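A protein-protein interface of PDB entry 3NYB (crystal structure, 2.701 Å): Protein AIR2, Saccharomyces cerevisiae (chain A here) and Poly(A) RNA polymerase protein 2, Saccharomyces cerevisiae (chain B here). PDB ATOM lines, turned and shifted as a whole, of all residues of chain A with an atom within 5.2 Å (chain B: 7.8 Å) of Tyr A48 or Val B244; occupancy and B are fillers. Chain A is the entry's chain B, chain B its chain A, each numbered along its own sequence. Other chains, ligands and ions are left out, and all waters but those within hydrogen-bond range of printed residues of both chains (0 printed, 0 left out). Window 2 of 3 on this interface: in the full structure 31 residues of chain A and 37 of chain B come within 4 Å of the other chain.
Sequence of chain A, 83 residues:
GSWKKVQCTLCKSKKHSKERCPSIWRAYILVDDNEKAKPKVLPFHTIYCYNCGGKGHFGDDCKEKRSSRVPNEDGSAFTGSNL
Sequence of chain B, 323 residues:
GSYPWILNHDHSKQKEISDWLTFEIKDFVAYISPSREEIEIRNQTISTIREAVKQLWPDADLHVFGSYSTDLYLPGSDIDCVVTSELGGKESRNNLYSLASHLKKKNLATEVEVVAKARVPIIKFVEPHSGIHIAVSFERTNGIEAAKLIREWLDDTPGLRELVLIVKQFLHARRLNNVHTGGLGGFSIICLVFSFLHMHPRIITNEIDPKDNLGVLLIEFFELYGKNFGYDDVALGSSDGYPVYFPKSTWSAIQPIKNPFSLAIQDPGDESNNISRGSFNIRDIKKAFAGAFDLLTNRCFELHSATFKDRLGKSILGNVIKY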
ATOM      1  N   THR A  46     -11.901   2.267  -0.246  1.00  0.00           N
ATOM      2  CA  THR A  46     -11.731   3.161  -1.385  1.00  0.00           C
ATOM      3  C   THR A  46     -12.542   4.442  -1.193  1.00  0.00           C
ATOM      4  O   THR A  46     -13.360   4.542  -0.281  1.00  0.00           O
ATOM      5  CB  THR A  46     -12.139   2.484  -2.708  1.00  0.00           C
ATOM      6  OG1 THR A  46     -11.808   1.092  -2.658  1.00  0.00           O
ATOM      7  CG2 THR A  46     -11.420   3.131  -3.887  1.00  0.00           C
ATOM      8  N   ILE A  47     -12.303   5.419  -2.057  1.00  0.00           N
ATOM      9  CA  ILE A  47     -12.925   6.726  -1.944  1.00  0.00           C
ATOM     10  C   ILE A  47     -14.014   6.843  -3.000  1.00  0.00           C
ATOM     11  O   ILE A  47     -13.990   6.121  -3.993  1.00  0.00           O
ATOM     12  CB  ILE A  47     -11.881   7.849  -2.126  1.00  0.00           C
ATOM     13  CG1 ILE A  47     -10.939   7.900  -0.925  1.00  0.00           C
ATOM     14  CG2 ILE A  47     -12.547   9.197  -2.307  1.00  0.00           C
ATOM     15  CD1 ILE A  47      -9.861   6.833  -0.938  1.00  0.00           C
ATOM     16  N   TYR A  48     -14.976   7.732  -2.778  1.00  0.00           N
ATOM     17  CA  TYR A  48     -16.045   7.939  -3.745  1.00  0.00           C
ATOM     18  C   TYR A  48     -16.376   9.410  -3.916  1.00  0.00           C
ATOM     19  O   TYR A  48     -16.447  10.160  -2.949  1.00  0.00           O
ATOM     20  CB  TYR A  48     -17.283   7.149  -3.349  1.00  0.00           C
ATOM     21  CG  TYR A  48     -17.087   5.659  -3.437  1.00  0.00           C
ATOM     22  CD1 TYR A  48     -16.632   4.934  -2.346  1.00  0.00           C
ATOM     23  CD2 TYR A  48     -17.349   4.975  -4.614  1.00  0.00           C
ATOM     24  CE1 TYR A  48     -16.449   3.567  -2.420  1.00  0.00           C
ATOM     25  CE2 TYR A  48     -17.169   3.606  -4.699  1.00  0.00           C
ATOM     26  CZ  TYR A  48     -16.718   2.908  -3.599  1.00  0.00           C
ATOM     27  OH  TYR A  48     -16.538   1.547  -3.677  1.00  0.00           O
ATOM     28  N   CYS A  49     -16.576   9.813  -5.164  1.00  0.00           N
ATOM     29  CA  CYS A  49     -16.807  11.207  -5.484  1.00  0.00           C
ATOM     30  C   CYS A  49     -18.291  11.530  -5.568  1.00  0.00           C
ATOM     31  O   CYS A  49     -19.055  10.831  -6.231  1.00  0.00           O
ATOM     32  CB  CYS A  49     -16.123  11.556  -6.797  1.00  0.00           C
ATOM     33  SG  CYS A  49     -16.718  13.086  -7.497  1.00  0.00           S
ATOM     34  N   TYR A  50     -18.695  12.601  -4.899  1.00  0.00           N
ATOM     35  CA  TYR A  50     -20.101  12.956  -4.827  1.00  0.00           C
ATOM     36  C   TYR A  50     -20.580  13.629  -6.099  1.00  0.00           C
ATOM     37  O   TYR A  50     -21.780  13.787  -6.318  1.00  0.00           O
ATOM     38  CB  TYR A  50     -20.374  13.840  -3.611  1.00  0.00           C
ATOM     39  CG  TYR A  50     -19.708  15.202  -3.607  1.00  0.00           C
ATOM     40  CD1 TYR A  50     -19.975  16.139  -4.597  1.00  0.00           C
ATOM     41  CD2 TYR A  50     -18.851  15.569  -2.579  1.00  0.00           C
ATOM     42  CE1 TYR A  50     -19.385  17.391  -4.575  1.00  0.00           C
ATOM     43  CE2 TYR A  50     -18.256  16.815  -2.548  1.00  0.00           C
ATOM     44  CZ  TYR A  50     -18.524  17.724  -3.546  1.00  0.00           C
ATOM     45  OH  TYR A  50     -17.927  18.965  -3.507  1.00  0.00           O
ATOM     46  N   GLY A  53     -20.137   9.471  -9.881  1.00  0.00           N
ATOM     47  CA  GLY A  53     -20.160   8.274  -9.061  1.00  0.00           C
ATOM     48  C   GLY A  53     -18.853   7.508  -9.089  1.00  0.00           C
ATOM     49  O   GLY A  53     -18.814   6.327  -8.758  1.00  0.00           O
ATOM     50  N   GLY A  54     -17.777   8.185  -9.476  1.00  0.00           N
ATOM     51  CA  GLY A  54     -16.483   7.550  -9.649  1.00  0.00           C
ATOM     52  C   GLY A  54     -15.691   7.345  -8.371  1.00  0.00           C
ATOM     53  O   GLY A  54     -15.825   8.108  -7.413  1.00  0.00           O
ATOM     54  N   LYS A  55     -14.852   6.313  -8.369  1.00  0.00           N
ATOM     55  CA  LYS A  55     -14.039   5.970  -7.203  1.00  0.00           C
ATOM     56  C   LYS A  55     -12.610   6.479  -7.338  1.00  0.00           C
ATOM     57  O   LYS A  55     -12.136   6.729  -8.444  1.00  0.00           O
ATOM     58  CB  LYS A  55     -14.030   4.457  -6.991  1.00  0.00           C
ATOM     59  CG  LYS A  55     -13.450   3.684  -8.149  1.00  0.00           C
ATOM     60  CD  LYS A  55     -14.175   2.364  -8.359  1.00  0.00           C
ATOM     61  CE  LYS A  55     -14.176   1.509  -7.107  1.00  0.00           C
ATOM     62  NZ  LYS A  55     -14.864   0.215  -7.361  1.00  0.00           N
ATOM     63  N   GLY A  56     -11.934   6.640  -6.203  1.00  0.00           N
ATOM     64  CA  GLY A  56     -10.540   7.042  -6.187  1.00  0.00           C
ATOM     65  C   GLY A  56     -10.282   8.497  -5.841  1.00  0.00           C
ATOM     66  O   GLY A  56      -9.130   8.901  -5.696  1.00  0.00           O
ATOM     67  N   HIS A  57     -11.341   9.290  -5.709  1.00  0.00           N
ATOM     68  CA  HIS A  57     -11.189  10.706  -5.381  1.00  0.00           C
ATOM     69  C   HIS A  57     -12.470  11.290  -4.789  1.00  0.00           C
ATOM     70  O   HIS A  57     -13.561  10.766  -5.011  1.00  0.00           O
ATOM     71  CB  HIS A  57     -10.788  11.498  -6.627  1.00  0.00           C
ATOM     72  CG  HIS A  57     -11.861  11.572  -7.664  1.00  0.00           C
ATOM     73  ND1 HIS A  57     -12.136  10.529  -8.533  1.00  0.00           N
ATOM     74  CD2 HIS A  57     -12.735  12.554  -7.981  1.00  0.00           C
ATOM     75  CE1 HIS A  57     -13.125  10.872  -9.329  1.00  0.00           C
ATOM     76  NE2 HIS A  57     -13.513  12.098  -9.015  1.00  0.00           N
ATOM     77  N   PHE A  58     -12.330  12.383  -4.046  1.00  0.00           N
ATOM     78  CA  PHE A  58     -13.478  13.049  -3.442  1.00  0.00           C
ATOM     79  C   PHE A  58     -14.236  13.935  -4.422  1.00  0.00           C
ATOM     80  O   PHE A  58     -13.650  14.529  -5.322  1.00  0.00           O
ATOM     81  CB  PHE A  58     -13.040  13.884  -2.245  1.00  0.00           C
ATOM     82  CG  PHE A  58     -12.572  13.070  -1.082  1.00  0.00           C
ATOM     83  CD1 PHE A  58     -13.397  12.114  -0.515  1.00  0.00           C
ATOM     84  CD2 PHE A  58     -11.313  13.267  -0.546  1.00  0.00           C
ATOM     85  CE1 PHE A  58     -12.972  11.361   0.562  1.00  0.00           C
ATOM     86  CE2 PHE A  58     -10.882  12.520   0.530  1.00  0.00           C
ATOM     87  CZ  PHE A  58     -11.717  11.563   1.087  1.00  0.00           C
ATOM     88  N   GLY A  59     -15.545  14.034  -4.221  1.00  0.00           N
ATOM     89  CA  GLY A  59     -16.393  14.842  -5.078  1.00  0.00           C
ATOM     90  C   GLY A  59     -16.001  16.305  -5.140  1.00  0.00           C
ATOM     91  O   GLY A  59     -16.401  17.032  -6.051  1.00  0.00           O
ATOM     92  N   CYS B 191     -29.868   5.689   5.436  1.00  0.00           N
ATOM     93  CA  CYS B 191     -28.840   5.479   4.424  1.00  0.00           C
ATOM     94  C   CYS B 191     -27.926   6.690   4.245  1.00  0.00           C
ATOM     95  O   CYS B 191     -26.705   6.566   4.337  1.00  0.00           O
ATOM     96  CB  CYS B 191     -29.458   5.097   3.082  1.00  0.00           C
ATOM     97  SG  CYS B 191     -28.223   4.732   1.841  1.00  0.00           S
ATOM     98  N   PHE B 194     -25.712   7.252   7.208  1.00  0.00           N
ATOM     99  CA  PHE B 194     -24.773   6.150   7.306  1.00  0.00           C
ATOM    100  C   PHE B 194     -23.647   6.309   6.291  1.00  0.00           C
ATOM    101  O   PHE B 194     -22.469   6.272   6.646  1.00  0.00           O
ATOM    102  CB  PHE B 194     -25.488   4.821   7.098  1.00  0.00           C
ATOM    103  CG  PHE B 194     -24.559   3.654   6.922  1.00  0.00           C
ATOM    104  CD1 PHE B 194     -23.613   3.354   7.890  1.00  0.00           C
ATOM    105  CD2 PHE B 194     -24.639   2.851   5.794  1.00  0.00           C
ATOM    106  CE1 PHE B 194     -22.761   2.282   7.732  1.00  0.00           C
ATOM    107  CE2 PHE B 194     -23.796   1.782   5.630  1.00  0.00           C
ATOM    108  CZ  PHE B 194     -22.854   1.494   6.600  1.00  0.00           C
ATOM    109  N   SER B 195     -24.021   6.491   5.028  1.00  0.00           N
ATOM    110  CA  SER B 195     -23.050   6.687   3.976  1.00  0.00           C
ATOM    111  C   SER B 195     -22.091   7.807   4.363  1.00  0.00           C
ATOM    112  O   SER B 195     -20.880   7.590   4.491  1.00  0.00           O
ATOM    113  CB  SER B 195     -23.755   7.027   2.670  1.00  0.00           C
ATOM    114  OG  SER B 195     -22.879   7.702   1.788  1.00  0.00           O
ATOM    115  N   HIS B 198     -19.624   6.981   7.103  1.00  0.00           N
ATOM    116  CA  HIS B 198     -18.642   5.948   6.801  1.00  0.00           C
ATOM    117  C   HIS B 198     -17.600   6.335   5.768  1.00  0.00           C
ATOM    118  O   HIS B 198     -16.540   5.714   5.701  1.00  0.00           O
ATOM    119  CB  HIS B 198     -19.319   4.634   6.423  1.00  0.00           C
ATOM    120  CG  HIS B 198     -19.256   3.600   7.494  1.00  0.00           C
ATOM    121  ND1 HIS B 198     -19.250   3.923   8.843  1.00  0.00           N
ATOM    122  CD2 HIS B 198     -19.191   2.250   7.444  1.00  0.00           C
ATOM    123  CE1 HIS B 198     -19.187   2.823   9.559  1.00  0.00           C
ATOM    124  NE2 HIS B 198     -19.152   1.785   8.733  1.00  0.00           N
ATOM    125  N   MET B 199     -17.881   7.355   4.968  1.00  0.00           N
ATOM    126  CA  MET B 199     -16.881   7.790   4.001  1.00  0.00           C
ATOM    127  C   MET B 199     -16.450   9.246   4.164  1.00  0.00           C
ATOM    128  O   MET B 199     -16.206   9.950   3.191  1.00  0.00           O
ATOM    129  CB  MET B 199     -17.336   7.502   2.574  1.00  0.00           C
ATOM    130  CG  MET B 199     -18.685   8.031   2.218  1.00  0.00           C
ATOM    131  SD  MET B 199     -19.059   7.602   0.516  1.00  0.00           S
ATOM    132  CE  MET B 199     -17.809   8.559  -0.331  1.00  0.00           C
ATOM    133  N   PHE B 229     -23.937  17.263  -3.313  1.00  0.00           N
ATOM    134  CA  PHE B 229     -24.193  15.925  -3.823  1.00  0.00           C
ATOM    135  C   PHE B 229     -24.764  15.974  -5.241  1.00  0.00           C
ATOM    136  O   PHE B 229     -25.734  16.680  -5.513  1.00  0.00           O
ATOM    137  CB  PHE B 229     -25.093  15.126  -2.882  1.00  0.00           C
ATOM    138  CG  PHE B 229     -25.203  13.668  -3.247  1.00  0.00           C
ATOM    139  CD1 PHE B 229     -24.288  12.749  -2.774  1.00  0.00           C
ATOM    140  CD2 PHE B 229     -26.224  13.221  -4.073  1.00  0.00           C
ATOM    141  CE1 PHE B 229     -24.390  11.402  -3.117  1.00  0.00           C
ATOM    142  CE2 PHE B 229     -26.332  11.880  -4.419  1.00  0.00           C
ATOM    143  CZ  PHE B 229     -25.410  10.971  -3.939  1.00  0.00           C
ATOM    144  N   VAL B 234     -25.156  10.869  -9.331  1.00  0.00           N
ATOM    145  CA  VAL B 234     -24.624   9.905  -8.364  1.00  0.00           C
ATOM    146  C   VAL B 234     -25.697   9.105  -7.622  1.00  0.00           C
ATOM    147  O   VAL B 234     -26.701   9.660  -7.184  1.00  0.00           O
ATOM    148  CB  VAL B 234     -23.723  10.594  -7.325  1.00  0.00           C
ATOM    149  CG1 VAL B 234     -23.036   9.560  -6.446  1.00  0.00           C
ATOM    150  CG2 VAL B 234     -22.702  11.474  -8.013  1.00  0.00           C
ATOM    151  N   ALA B 235     -25.467   7.803  -7.469  1.00  0.00           N
ATOM    152  CA  ALA B 235     -26.391   6.926  -6.749  1.00  0.00           C
ATOM    153  C   ALA B 235     -25.718   6.294  -5.534  1.00  0.00           C
ATOM    154  O   ALA B 235     -24.494   6.331  -5.407  1.00  0.00           O
ATOM    155  CB  ALA B 235     -26.927   5.844  -7.674  1.00  0.00           C
ATOM    156  N   LEU B 236     -26.519   5.715  -4.642  1.00  0.00           N
ATOM    157  CA  LEU B 236     -25.981   5.092  -3.438  1.00  0.00           C
ATOM    158  C   LEU B 236     -26.305   3.612  -3.382  1.00  0.00           C
ATOM    159  O   LEU B 236     -27.415   3.203  -3.720  1.00  0.00           O
ATOM    160  CB  LEU B 236     -26.514   5.772  -2.173  1.00  0.00           C
ATOM    161  CG  LEU B 236     -25.933   7.128  -1.791  1.00  0.00           C
ATOM    162  CD1 LEU B 236     -26.643   8.194  -2.553  1.00  0.00           C
ATOM    163  CD2 LEU B 236     -26.106   7.348  -0.312  1.00  0.00           C
ATOM    164  N   GLY B 237     -25.331   2.820  -2.937  1.00  0.00           N
ATOM    165  CA  GLY B 237     -25.502   1.387  -2.785  1.00  0.00           C
ATOM    166  C   GLY B 237     -24.546   0.817  -1.755  1.00  0.00           C
ATOM    167  O   GLY B 237     -23.856   1.564  -1.061  1.00  0.00           O
ATOM    168  N   SER B 238     -24.507  -0.509  -1.655  1.00  0.00           N
ATOM    169  CA  SER B 238     -23.632  -1.183  -0.700  1.00  0.00           C
ATOM    170  C   SER B 238     -23.008  -2.450  -1.270  1.00  0.00           C
ATOM    171  O   SER B 238     -23.665  -3.486  -1.392  1.00  0.00           O
ATOM    172  CB  SER B 238     -24.377  -1.506   0.598  1.00  0.00           C
ATOM    173  OG  SER B 238     -24.170  -0.499   1.573  1.00  0.00           O
ATOM    174  N   SER B 239     -21.730  -2.355  -1.616  1.00  0.00           N
ATOM    175  CA  SER B 239     -20.959  -3.513  -2.034  1.00  0.00           C
ATOM    176  C   SER B 239     -20.170  -4.038  -0.848  1.00  0.00           C
ATOM    177  O   SER B 239     -19.133  -3.487  -0.493  1.00  0.00           O
ATOM    178  CB  SER B 239     -20.006  -3.146  -3.170  1.00  0.00           C
ATOM    179  OG  SER B 239     -19.122  -4.216  -3.455  1.00  0.00           O
ATOM    180  N   ASP B 240     -20.682  -5.095  -0.229  1.00  0.00           N
ATOM    181  CA  ASP B 240     -19.996  -5.743   0.883  1.00  0.00           C
ATOM    182  C   ASP B 240     -20.010  -4.888   2.144  1.00  0.00           C
ATOM    183  O   ASP B 240     -18.957  -4.566   2.694  1.00  0.00           O
ATOM    184  CB  ASP B 240     -18.553  -6.079   0.498  1.00  0.00           C
ATOM    185  CG  ASP B 240     -18.454  -6.728  -0.869  1.00  0.00           C
ATOM    186  OD1 ASP B 240     -19.457  -7.322  -1.321  1.00  0.00           O
ATOM    187  OD2 ASP B 240     -17.373  -6.641  -1.491  1.00  0.00           O
ATOM    188  N   GLY B 241     -21.206  -4.526   2.597  1.00  0.00           N
ATOM    189  CA  GLY B 241     -21.366  -3.748   3.814  1.00  0.00           C
ATOM    190  C   GLY B 241     -20.576  -2.455   3.796  1.00  0.00           C
ATOM    191  O   GLY B 241     -20.315  -1.855   4.838  1.00  0.00           O
ATOM    192  N   TYR B 242     -20.186  -2.031   2.599  1.00  0.00           N
ATOM    193  CA  TYR B 242     -19.455  -0.785   2.422  1.00  0.00           C
ATOM    194  C   TYR B 242     -20.278   0.202   1.603  1.00  0.00           C
ATOM    195  O   TYR B 242     -20.626  -0.081   0.459  1.00  0.00           O
ATOM    196  CB  TYR B 242     -18.121  -1.043   1.717  1.00  0.00           C
ATOM    197  CG  TYR B 242     -16.983  -1.441   2.631  1.00  0.00           C
ATOM    198  CD1 TYR B 242     -16.374  -0.507   3.458  1.00  0.00           C
ATOM    199  CD2 TYR B 242     -16.500  -2.743   2.648  1.00  0.00           C
ATOM    200  CE1 TYR B 242     -15.326  -0.860   4.289  1.00  0.00           C
ATOM    201  CE2 TYR B 242     -15.452  -3.107   3.475  1.00  0.00           C
ATOM    202  CZ  TYR B 242     -14.868  -2.161   4.294  1.00  0.00           C
ATOM    203  OH  TYR B 242     -13.824  -2.515   5.120  1.00  0.00           O
ATOM    204  N   PRO B 243     -20.605   1.361   2.193  1.00  0.00           N
ATOM    205  CA  PRO B 243     -21.286   2.440   1.472  1.00  0.00           C
ATOM    206  C   PRO B 243     -20.528   2.822   0.203  1.00  0.00           C
ATOM    207  O   PRO B 243     -19.299   2.893   0.209  1.00  0.00           O
ATOM    208  CB  PRO B 243     -21.263   3.598   2.481  1.00  0.00           C
ATOM    209  CG  PRO B 243     -20.254   3.187   3.522  1.00  0.00           C
ATOM    210  CD  PRO B 243     -20.416   1.714   3.606  1.00  0.00           C
ATOM    211  N   VAL B 244     -21.267   3.077  -0.871  1.00  0.00           N
ATOM    212  CA  VAL B 244     -20.681   3.216  -2.197  1.00  0.00           C
ATOM    213  C   VAL B 244     -21.461   4.203  -3.054  1.00  0.00           C
ATOM    214  O   VAL B 244     -22.686   4.251  -2.988  1.00  0.00           O
ATOM    215  CB  VAL B 244     -20.681   1.848  -2.913  1.00  0.00           C
ATOM    216  CG1 VAL B 244     -20.918   2.009  -4.407  1.00  0.00           C
ATOM    217  CG2 VAL B 244     -19.399   1.102  -2.631  1.00  0.00           C
ATOM    218  N   TYR B 245     -20.756   5.001  -3.850  1.00  0.00           N
ATOM    219  CA  TYR B 245     -21.408   5.759  -4.910  1.00  0.00           C
ATOM    220  C   TYR B 245     -21.181   5.056  -6.239  1.00  0.00           C
ATOM    221  O   TYR B 245     -20.117   4.484  -6.474  1.00  0.00           O
ATOM    222  CB  TYR B 245     -20.845   7.176  -5.040  1.00  0.00           C
ATOM    223  CG  TYR B 245     -20.902   8.046  -3.809  1.00  0.00           C
ATOM    224  CD1 TYR B 245     -21.833   7.823  -2.805  1.00  0.00           C
ATOM    225  CD2 TYR B 245     -20.040   9.125  -3.674  1.00  0.00           C
ATOM    226  CE1 TYR B 245     -21.880   8.637  -1.680  1.00  0.00           C
ATOM    227  CE2 TYR B 245     -20.082   9.944  -2.561  1.00  0.00           C
ATOM    228  CZ  TYR B 245     -21.002   9.696  -1.565  1.00  0.00           C
ATOM    229  OH  TYR B 245     -21.034  10.515  -0.460  1.00  0.00           O
ATOM    230  N   PHE B 246     -22.175   5.099  -7.115  1.00  0.00           N
ATOM    231  CA  PHE B 246     -21.946   4.737  -8.507  1.00  0.00           C
ATOM    232  C   PHE B 246     -22.737   5.647  -9.434  1.00  0.00           C
ATOM    233  O   PHE B 246     -23.799   6.132  -9.061  1.00  0.00           O
ATOM    234  CB  PHE B 246     -22.223   3.249  -8.778  1.00  0.00           C
ATOM    235  CG  PHE B 246     -23.595   2.783  -8.376  1.00  0.00           C
ATOM    236  CD1 PHE B 246     -24.647   2.826  -9.273  1.00  0.00           C
ATOM    237  CD2 PHE B 246     -23.817   2.253  -7.114  1.00  0.00           C
ATOM    238  CE1 PHE B 246     -25.905   2.378  -8.909  1.00  0.00           C
ATOM    239  CE2 PHE B 246     -25.071   1.803  -6.747  1.00  0.00           C
ATOM    240  CZ  PHE B 246     -26.117   1.867  -7.645  1.00  0.00           C
ATOM    241  N   PRO B 247     -22.207   5.901 -10.643  1.00  0.00           N
ATOM    242  CA  PRO B 247     -22.854   6.840 -11.566  1.00  0.00           C
ATOM    243  C   PRO B 247     -24.167   6.261 -12.089  1.00  0.00           C
ATOM    244  O   PRO B 247     -24.265   5.054 -12.298  1.00  0.00           O
ATOM    245  CB  PRO B 247     -21.832   6.981 -12.705  1.00  0.00           C
ATOM    246  CG  PRO B 247     -20.561   6.333 -12.201  1.00  0.00           C
ATOM    247  CD  PRO B 247     -21.000   5.296 -11.231  1.00  0.00           C
ATOM    248  N   ALA B 264     -31.461   8.508  -5.832  1.00  0.00           N
ATOM    249  CA  ALA B 264     -31.366   7.110  -6.240  1.00  0.00           C
ATOM    250  C   ALA B 264     -30.545   6.304  -5.253  1.00  0.00           C
ATOM    251  O   ALA B 264     -29.326   6.446  -5.170  1.00  0.00           O
ATOM    252  CB  ALA B 264     -30.774   7.002  -7.617  1.00  0.00           C
ATOM    253  N   GLN B 266     -29.974   2.304  -3.972  1.00  0.00           N
ATOM    254  CA  GLN B 266     -30.194   0.924  -4.386  1.00  0.00           C
ATOM    255  C   GLN B 266     -30.993   0.127  -3.363  1.00  0.00           C
ATOM    256  O   GLN B 266     -30.595   0.013  -2.199  1.00  0.00           O
ATOM    257  CB  GLN B 266     -28.856   0.238  -4.655  1.00  0.00           C
ATOM    258  CG  GLN B 266     -28.972  -1.042  -5.452  1.00  0.00           C
ATOM    259  CD  GLN B 266     -27.673  -1.420  -6.120  1.00  0.00           C
ATOM    260  OE1 GLN B 266     -26.643  -1.577  -5.457  1.00  0.00           O
ATOM    261  NE2 GLN B 266     -27.709  -1.572  -7.444  1.00  0.00           N
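The backbone carbonyl oxygen of Tyr B245 sits close to the backbone carbonyl oxygen of Gly A53 (3.2 Å).
SG of Cys A49 lies close to N of Gly A59 (3.6 Å). The backbone NH (N) of Val B244 is in hydrogen-bond range of the backbone carbonyl oxygen (O) of Gly B237 (3.0 Å). SD of Met B199 lies close to OH of Tyr B245. The backbone carbonyl oxygen (O) of Phe B246 is in hydrogen-bond range of the backbone NH (N) of Ala B235 (2.8 Å). The backbone NH (N) of Cys A49 is in hydrogen-bond range of the backbone carbonyl oxygen (O) of Gly A54 (2.9 Å).
Among the printed residues, pairs that only touch across the chains: Tyr A50 with Val B234 (3.0 Å), Tyr A48 with Val B244 (3.1 Å), Cys A49 with Tyr B245 (3.2 Å), Tyr A48 with Met B199 (3.4 Å), Tyr A48 with Tyr B245 (3.4 Å), Gly A53 with Pro B247 (3.5 Å), Gly A53 with Phe B246 (3.5 Å), Gly A53 with Val B234 (3.8 Å), Tyr A50 with Tyr B245 (3.8 Å), Tyr A50 with Phe B229 (3.9 Å) and Tyr A48 with Pro B243 (3.9 Å).
Printed residues of chain B within 4 Å of Tyr A48: Met B199 (3.4 Å), Pro B243 (3.9 Å), Val B244 (3.1 Å) and Tyr B245 (3.4 Å). Of chain A, only Tyr A48 (3.1 Å) comes within 4 Å of Val B244. Of the printed residues of chain A, Pro B243 touches Tyr A48 (3.9 Å). Of the printed residues of chain B, Cys A49 touches Tyr B245 (3.2 Å). Of the printed residues of chain B, Gly A53 touches Val B234, Tyr B245, Phe B246 and Pro B247. Of the printed residues of chain A, Tyr B245 touches Tyr A48, Cys A49, Tyr A50 and Gly A53. The nearest printed residue of chain A that does not touch Val B244 is Gly A53 (6.5 Å). The nearest printed residue of chain B that does not touch Tyr A50 is Met B199 (6.2 Å).
Of the 22 printed residues of chain B, 8 touch a printed residue of chain A. Hydrophobic or aromatic side chains of chain B within 4 Å of the printed part of chain A: Met B199, Val B234, Val B244, Tyr B245 and Pro B247. Printed residues of chain A that touch a printed residue of chain B: Tyr A48, Cys A49, Tyr A50 and Gly A53. Among the printed residues, 12 pairs touch across the chains.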
